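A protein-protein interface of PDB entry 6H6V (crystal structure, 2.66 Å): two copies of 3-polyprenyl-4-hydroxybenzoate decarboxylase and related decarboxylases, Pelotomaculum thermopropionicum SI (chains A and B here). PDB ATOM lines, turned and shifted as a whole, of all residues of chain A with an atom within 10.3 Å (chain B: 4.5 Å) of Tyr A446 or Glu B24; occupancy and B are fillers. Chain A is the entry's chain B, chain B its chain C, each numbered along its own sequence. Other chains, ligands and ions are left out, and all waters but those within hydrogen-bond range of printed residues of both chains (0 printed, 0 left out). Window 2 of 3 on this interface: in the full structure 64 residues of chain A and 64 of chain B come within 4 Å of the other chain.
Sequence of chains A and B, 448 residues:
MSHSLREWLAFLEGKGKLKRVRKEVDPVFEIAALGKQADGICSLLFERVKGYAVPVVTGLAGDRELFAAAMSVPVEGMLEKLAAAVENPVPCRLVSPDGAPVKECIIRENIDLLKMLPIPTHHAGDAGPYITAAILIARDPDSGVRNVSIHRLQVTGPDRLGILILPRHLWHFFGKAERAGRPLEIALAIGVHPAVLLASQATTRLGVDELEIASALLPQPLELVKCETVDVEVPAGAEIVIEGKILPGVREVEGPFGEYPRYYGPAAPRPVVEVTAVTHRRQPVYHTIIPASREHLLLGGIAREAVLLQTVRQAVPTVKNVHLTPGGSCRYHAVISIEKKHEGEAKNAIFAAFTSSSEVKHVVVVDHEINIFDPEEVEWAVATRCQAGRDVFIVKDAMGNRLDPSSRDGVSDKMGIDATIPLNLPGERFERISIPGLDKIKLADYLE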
ATOM      1  N   GLY A 437     -16.134  -4.151 -20.562  1.00  0.00           N
ATOM      2  CA  GLY A 437     -15.972  -2.750 -20.209  1.00  0.00           C
ATOM      3  C   GLY A 437     -17.092  -2.131 -19.408  1.00  0.00           C
ATOM      4  O   GLY A 437     -17.203  -0.919 -19.379  1.00  0.00           O
ATOM      5  N   LEU A 438     -17.913  -2.944 -18.758  1.00  0.00           N
ATOM      6  CA  LEU A 438     -19.050  -2.424 -17.945  1.00  0.00           C
ATOM      7  C   LEU A 438     -18.549  -1.703 -16.690  1.00  0.00           C
ATOM      8  O   LEU A 438     -19.025  -0.623 -16.368  1.00  0.00           O
ATOM      9  CB  LEU A 438     -20.046  -3.532 -17.585  1.00  0.00           C
ATOM     10  CG  LEU A 438     -21.075  -3.255 -16.460  1.00  0.00           C
ATOM     11  CD1 LEU A 438     -22.114  -2.258 -16.935  1.00  0.00           C
ATOM     12  CD2 LEU A 438     -21.695  -4.521 -15.917  1.00  0.00           C
ATOM     13  N   ASP A 439     -17.602  -2.313 -15.985  1.00  0.00           N
ATOM     14  CA  ASP A 439     -17.094  -1.721 -14.737  1.00  0.00           C
ATOM     15  C   ASP A 439     -16.217  -0.513 -15.025  1.00  0.00           C
ATOM     16  O   ASP A 439     -16.154   0.426 -14.246  1.00  0.00           O
ATOM     17  CB  ASP A 439     -16.288  -2.765 -13.944  1.00  0.00           C
ATOM     18  CG  ASP A 439     -17.124  -3.946 -13.494  1.00  0.00           C
ATOM     19  OD1 ASP A 439     -18.130  -3.713 -12.789  1.00  0.00           O
ATOM     20  OD2 ASP A 439     -16.814  -5.103 -13.893  1.00  0.00           O
ATOM     21  N   LYS A 440     -15.549  -0.545 -16.172  1.00  0.00           N
ATOM     22  CA  LYS A 440     -14.753   0.569 -16.680  1.00  0.00           C
ATOM     23  C   LYS A 440     -15.598   1.808 -17.049  1.00  0.00           C
ATOM     24  O   LYS A 440     -15.142   2.923 -16.861  1.00  0.00           O
ATOM     25  CB  LYS A 440     -13.911   0.051 -17.874  1.00  0.00           C
ATOM     26  CG  LYS A 440     -13.356   1.057 -18.884  1.00  0.00           C
ATOM     27  CD  LYS A 440     -11.888   1.397 -18.648  1.00  0.00           C
ATOM     28  CE  LYS A 440     -11.501   2.657 -19.400  1.00  0.00           C
ATOM     29  NZ  LYS A 440     -10.258   3.218 -18.827  1.00  0.00           N
ATOM     30  N   ILE A 441     -16.796   1.616 -17.598  1.00  0.00           N
ATOM     31  CA  ILE A 441     -17.657   2.728 -18.044  1.00  0.00           C
ATOM     32  C   ILE A 441     -18.635   3.107 -16.937  1.00  0.00           C
ATOM     33  O   ILE A 441     -19.047   2.266 -16.133  1.00  0.00           O
ATOM     34  CB  ILE A 441     -18.396   2.385 -19.367  1.00  0.00           C
ATOM     35  CG1 ILE A 441     -18.644   3.642 -20.210  1.00  0.00           C
ATOM     36  CG2 ILE A 441     -19.718   1.657 -19.110  1.00  0.00           C
ATOM     37  CD1 ILE A 441     -19.121   3.298 -21.613  1.00  0.00           C
ATOM     38  N   LYS A 442     -19.001   4.384 -16.889  1.00  0.00           N
ATOM     39  CA  LYS A 442     -19.826   4.902 -15.802  1.00  0.00           C
ATOM     40  C   LYS A 442     -20.873   5.848 -16.411  1.00  0.00           C
ATOM     41  O   LYS A 442     -20.528   6.789 -17.116  1.00  0.00           O
ATOM     42  CB  LYS A 442     -18.905   5.593 -14.815  1.00  0.00           C
ATOM     43  CG  LYS A 442     -19.512   5.932 -13.460  1.00  0.00           C
ATOM     44  CD  LYS A 442     -19.332   4.819 -12.436  1.00  0.00           C
ATOM     45  CE  LYS A 442     -19.473   5.364 -11.011  1.00  0.00           C
ATOM     46  NZ  LYS A 442     -20.718   6.169 -10.768  1.00  0.00           N
ATOM     47  N   LEU A 443     -22.151   5.578 -16.148  1.00  0.00           N
ATOM     48  CA  LEU A 443     -23.261   6.308 -16.796  1.00  0.00           C
ATOM     49  C   LEU A 443     -23.278   7.791 -16.441  1.00  0.00           C
ATOM     50  O   LEU A 443     -23.537   8.612 -17.313  1.00  0.00           O
ATOM     51  CB  LEU A 443     -24.625   5.681 -16.435  1.00  0.00           C
ATOM     52  CG  LEU A 443     -25.883   6.368 -17.008  1.00  0.00           C
ATOM     53  CD1 LEU A 443     -25.999   6.182 -18.513  1.00  0.00           C
ATOM     54  CD2 LEU A 443     -27.140   5.903 -16.303  1.00  0.00           C
ATOM     55  N   ALA A 444     -23.016   8.129 -15.174  1.00  0.00           N
ATOM     56  CA  ALA A 444     -23.008   9.521 -14.704  1.00  0.00           C
ATOM     57  C   ALA A 444     -22.072  10.454 -15.508  1.00  0.00           C
ATOM     58  O   ALA A 444     -22.361  11.645 -15.640  1.00  0.00           O
ATOM     59  CB  ALA A 444     -22.697   9.575 -13.212  1.00  0.00           C
ATOM     60  N   ASP A 445     -20.994   9.905 -16.069  1.00  0.00           N
ATOM     61  CA  ASP A 445     -20.079  10.626 -16.998  1.00  0.00           C
ATOM     62  C   ASP A 445     -20.663  10.964 -18.379  1.00  0.00           C
ATOM     63  O   ASP A 445     -20.032  11.705 -19.137  1.00  0.00           O
ATOM     64  CB  ASP A 445     -18.781   9.806 -17.249  1.00  0.00           C
ATOM     65  CG  ASP A 445     -17.993   9.486 -15.969  1.00  0.00           C
ATOM     66  OD1 ASP A 445     -18.272  10.066 -14.895  1.00  0.00           O
ATOM     67  OD2 ASP A 445     -17.081   8.634 -16.047  1.00  0.00           O
ATOM     68  N   TYR A 446     -21.814  10.386 -18.727  1.00  0.00           N
ATOM     69  CA  TYR A 446     -22.414  10.543 -20.073  1.00  0.00           C
ATOM     70  C   TYR A 446     -23.722  11.368 -20.116  1.00  0.00           C
ATOM     71  O   TYR A 446     -24.171  11.725 -21.205  1.00  0.00           O
ATOM     72  CB  TYR A 446     -22.635   9.162 -20.700  1.00  0.00           C
ATOM     73  CG  TYR A 446     -21.391   8.469 -21.209  1.00  0.00           C
ATOM     74  CD1 TYR A 446     -20.503   7.852 -20.334  1.00  0.00           C
ATOM     75  CD2 TYR A 446     -21.108   8.417 -22.573  1.00  0.00           C
ATOM     76  CE1 TYR A 446     -19.370   7.183 -20.815  1.00  0.00           C
ATOM     77  CE2 TYR A 446     -19.977   7.763 -23.049  1.00  0.00           C
ATOM     78  CZ  TYR A 446     -19.122   7.128 -22.155  1.00  0.00           C
ATOM     79  OH  TYR A 446     -18.002   6.512 -22.635  1.00  0.00           O
ATOM     80  N   LEU A 447     -24.316  11.672 -18.957  1.00  0.00           N
ATOM     81  CA  LEU A 447     -25.466  12.595 -18.888  1.00  0.00           C
ATOM     82  C   LEU A 447     -25.076  13.898 -18.134  1.00  0.00           C
ATOM     83  O   LEU A 447     -24.911  13.885 -16.905  1.00  0.00           O
ATOM     84  CB  LEU A 447     -26.731  11.903 -18.318  1.00  0.00           C
ATOM     85  CG  LEU A 447     -26.680  10.658 -17.410  1.00  0.00           C
ATOM     86  CD1 LEU A 447     -26.610  11.022 -15.927  1.00  0.00           C
ATOM     87  CD2 LEU A 447     -27.908   9.796 -17.649  1.00  0.00           C
ATOM     88  N   ARG B  20     -31.191  11.877 -22.012  1.00  0.00           N
ATOM     89  CA  ARG B  20     -30.484  11.931 -23.278  1.00  0.00           C
ATOM     90  C   ARG B  20     -28.991  11.788 -23.022  1.00  0.00           C
ATOM     91  O   ARG B  20     -28.478  12.267 -22.013  1.00  0.00           O
ATOM     92  CB  ARG B  20     -30.783  13.243 -23.988  1.00  0.00           C
ATOM     93  CG  ARG B  20     -32.242  13.408 -24.366  1.00  0.00           C
ATOM     94  CD  ARG B  20     -32.605  14.854 -24.695  1.00  0.00           C
ATOM     95  NE  ARG B  20     -34.010  14.981 -25.098  1.00  0.00           N
ATOM     96  CZ  ARG B  20     -34.493  14.763 -26.328  1.00  0.00           C
ATOM     97  NH1 ARG B  20     -33.700  14.419 -27.340  1.00  0.00           N
ATOM     98  NH2 ARG B  20     -35.791  14.908 -26.560  1.00  0.00           N
ATOM     99  N   VAL B  21     -28.302  11.104 -23.924  1.00  0.00           N
ATOM    100  CA  VAL B  21     -26.870  10.898 -23.814  1.00  0.00           C
ATOM    101  C   VAL B  21     -26.258  11.564 -25.016  1.00  0.00           C
ATOM    102  O   VAL B  21     -26.310  11.035 -26.129  1.00  0.00           O
ATOM    103  CB  VAL B  21     -26.512   9.399 -23.756  1.00  0.00           C
ATOM    104  CG1 VAL B  21     -25.000   9.174 -23.924  1.00  0.00           C
ATOM    105  CG2 VAL B  21     -27.025   8.796 -22.454  1.00  0.00           C
ATOM    106  N   ARG B  22     -25.688  12.742 -24.768  1.00  0.00           N
ATOM    107  CA  ARG B  22     -25.156  13.609 -25.818  1.00  0.00           C
ATOM    108  C   ARG B  22     -23.754  13.182 -26.215  1.00  0.00           C
ATOM    109  O   ARG B  22     -23.381  13.336 -27.368  1.00  0.00           O
ATOM    110  CB  ARG B  22     -25.193  15.069 -25.368  1.00  0.00           C
ATOM    111  CG  ARG B  22     -26.570  15.474 -24.894  1.00  0.00           C
ATOM    112  CD  ARG B  22     -26.768  16.985 -24.838  1.00  0.00           C
ATOM    113  NE  ARG B  22     -28.184  17.337 -24.931  1.00  0.00           N
ATOM    114  CZ  ARG B  22     -29.106  17.172 -23.970  1.00  0.00           C
ATOM    115  NH1 ARG B  22     -30.381  17.499 -24.207  1.00  0.00           N
ATOM    116  NH2 ARG B  22     -28.775  16.694 -22.768  1.00  0.00           N
ATOM    117  N   LYS B  23     -23.001  12.621 -25.278  1.00  0.00           N
ATOM    118  CA  LYS B  23     -21.632  12.176 -25.562  1.00  0.00           C
ATOM    119  C   LYS B  23     -21.639  11.025 -26.572  1.00  0.00           C
ATOM    120  O   LYS B  23     -22.614  10.281 -26.646  1.00  0.00           O
ATOM    121  CB  LYS B  23     -20.879  11.827 -24.267  1.00  0.00           C
ATOM    122  CG  LYS B  23     -19.425  12.301 -24.271  1.00  0.00           C
ATOM    123  CD  LYS B  23     -18.791  12.259 -22.873  1.00  0.00           C
ATOM    124  CE  LYS B  23     -17.264  12.259 -22.946  1.00  0.00           C
ATOM    125  NZ  LYS B  23     -16.647  11.264 -22.020  1.00  0.00           N
ATOM    126  N   GLU B  24     -20.588  10.910 -27.380  1.00  0.00           N
ATOM    127  CA  GLU B  24     -20.531   9.858 -28.403  1.00  0.00           C
ATOM    128  C   GLU B  24     -20.431   8.499 -27.717  1.00  0.00           C
ATOM    129  O   GLU B  24     -19.774   8.385 -26.686  1.00  0.00           O
ATOM    130  CB  GLU B  24     -19.355  10.062 -29.376  1.00  0.00           C
ATOM    131  CG  GLU B  24     -19.566   9.366 -30.720  1.00  0.00           C
ATOM    132  CD  GLU B  24     -18.295   9.201 -31.555  1.00  0.00           C
ATOM    133  OE1 GLU B  24     -17.311   8.573 -31.089  1.00  0.00           O
ATOM    134  OE2 GLU B  24     -18.290   9.671 -32.716  1.00  0.00           O
ATOM    135  N   VAL B  25     -21.117   7.491 -28.268  1.00  0.00           N
ATOM    136  CA  VAL B  25     -21.083   6.101 -27.761  1.00  0.00           C
ATOM    137  C   VAL B  25     -20.944   5.090 -28.901  1.00  0.00           C
ATOM    138  O   VAL B  25     -21.551   5.236 -29.953  1.00  0.00           O
ATOM    139  CB  VAL B  25     -22.323   5.736 -26.922  1.00  0.00           C
ATOM    140  CG1 VAL B  25     -22.424   6.626 -25.693  1.00  0.00           C
ATOM    141  CG2 VAL B  25     -23.613   5.875 -27.727  1.00  0.00           C
ATOM    142  N   GLU B  30     -20.844  -0.380 -25.776  1.00  0.00           N
ATOM    143  CA  GLU B  30     -21.062   0.801 -24.912  1.00  0.00           C
ATOM    144  C   GLU B  30     -22.540   1.138 -24.712  1.00  0.00           C
ATOM    145  O   GLU B  30     -22.918   1.601 -23.633  1.00  0.00           O
ATOM    146  CB  GLU B  30     -20.307   2.037 -25.415  1.00  0.00           C
ATOM    147  CG  GLU B  30     -18.782   1.948 -25.284  1.00  0.00           C
ATOM    148  CD  GLU B  30     -18.038   3.269 -25.516  1.00  0.00           C
ATOM    149  OE1 GLU B  30     -18.658   4.305 -25.869  1.00  0.00           O
ATOM    150  OE2 GLU B  30     -16.804   3.261 -25.315  1.00  0.00           O
ATOM    151  N   LEU B  34     -24.121   1.058 -20.955  1.00  0.00           N
ATOM    152  CA  LEU B  34     -24.782   2.214 -20.359  1.00  0.00           C
ATOM    153  C   LEU B  34     -26.235   1.927 -20.065  1.00  0.00           C
ATOM    154  O   LEU B  34     -26.737   2.297 -19.008  1.00  0.00           O
ATOM    155  CB  LEU B  34     -24.653   3.449 -21.268  1.00  0.00           C
ATOM    156  CG  LEU B  34     -23.211   3.938 -21.388  1.00  0.00           C
ATOM    157  CD1 LEU B  34     -23.036   4.820 -22.617  1.00  0.00           C
ATOM    158  CD2 LEU B  34     -22.868   4.683 -20.097  1.00  0.00           C
ATOM    159  N   ARG B  48     -25.930  10.485 -30.165  1.00  0.00           N
ATOM    160  CA  ARG B  48     -24.714  10.440 -30.970  1.00  0.00           C
ATOM    161  C   ARG B  48     -24.083   9.039 -30.923  1.00  0.00           C
ATOM    162  O   ARG B  48     -23.345   8.698 -30.003  1.00  0.00           O
ATOM    163  CB  ARG B  48     -23.734  11.516 -30.463  1.00  0.00           C
ATOM    164  CG  ARG B  48     -22.661  11.956 -31.451  1.00  0.00           C
ATOM    165  CD  ARG B  48     -21.703  12.988 -30.847  1.00  0.00           C
ATOM    166  NE  ARG B  48     -21.300  14.028 -31.795  1.00  0.00           N
ATOM    167  CZ  ARG B  48     -22.044  15.086 -32.147  1.00  0.00           C
ATOM    168  NH1 ARG B  48     -23.269  15.283 -31.644  1.00  0.00           N
ATOM    169  NH2 ARG B  48     -21.561  15.976 -33.024  1.00  0.00           N
ATOM    170  N   LYS B  50     -21.547   6.530 -32.659  1.00  0.00           N
ATOM    171  CA  LYS B  50     -20.359   6.478 -33.512  1.00  0.00           C
ATOM    172  C   LYS B  50     -20.560   5.720 -34.834  1.00  0.00           C
ATOM    173  O   LYS B  50     -20.757   4.502 -34.854  1.00  0.00           O
ATOM    174  CB  LYS B  50     -19.172   5.915 -32.693  1.00  0.00           C
ATOM    175  CG  LYS B  50     -17.811   5.784 -33.394  1.00  0.00           C
ATOM    176  CD  LYS B  50     -17.543   4.322 -33.777  1.00  0.00           C
ATOM    177  CE  LYS B  50     -16.337   4.128 -34.665  1.00  0.00           C
ATOM    178  NZ  LYS B  50     -15.123   4.107 -33.816  1.00  0.00           N
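Of the printed residues of chain B, Ile A441 touches Glu B30. Of the printed residues of chain B, Leu A443 touches Leu B34. Of the printed residues of chain B, Asp A445 touches Lys B23. Printed residues of chain B within 4 Å of Tyr A446: Val B21, Lys B23, Glu B24, Val B25, Glu B30 and Leu B34. Val B21 touches just one residue of chain A: Tyr A446 (3.8 Å). Lys B23 touches two residues of chain A. Of the printed residues of chain A, Glu B30 touches Ile A441 (3.9 Å) and Tyr A446 (3.97 Å). No residue of chain A comes within 4 Å of Lys B50. The nearest printed residue of chain B that does not touch Tyr A446 is Arg B22 (4.004 Å).
No position is printed for both chains. Of the 9 pairs that touch across the chains among the printed residues, none has its exchanged pair printed and touching as well.
Of the 11 printed residues of chain A, 4 touch a printed residue of chain B. Hydrophobic or aromatic side chains of chain A that line the printed part of chain B: Ile A441, Leu A443 and Tyr A446. Of the 10 printed residues of chain B, 6 touch a printed residue of chain A. Printed residues of chain B that touch a printed residue of chain A: Val B21, Lys B23, Glu B24, Val B25, Glu B30 and Leu B34. Among the printed residues, 9 pairs touch across the chains.
O of Val B25 is in hydrogen-bond range of N of Lys B50 (3.0 Å). The backbone NH (N) of Val B25 sits at hydrogen-bond distance from the backbone carbonyl oxygen (O) of Arg B48 (3.1 Å).
Among the printed residues, merely in contact across the chains: Tyr A446 with Glu B24, Leu A443 with Leu B34, Tyr A446 with Val B25, Tyr A446 with Lys B23, Tyr A446 with Val B21, Ile A441 with Glu B30, Tyr A446 with Leu B34, Tyr A446 with Glu B30 and Asp A445 with Lys B23.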
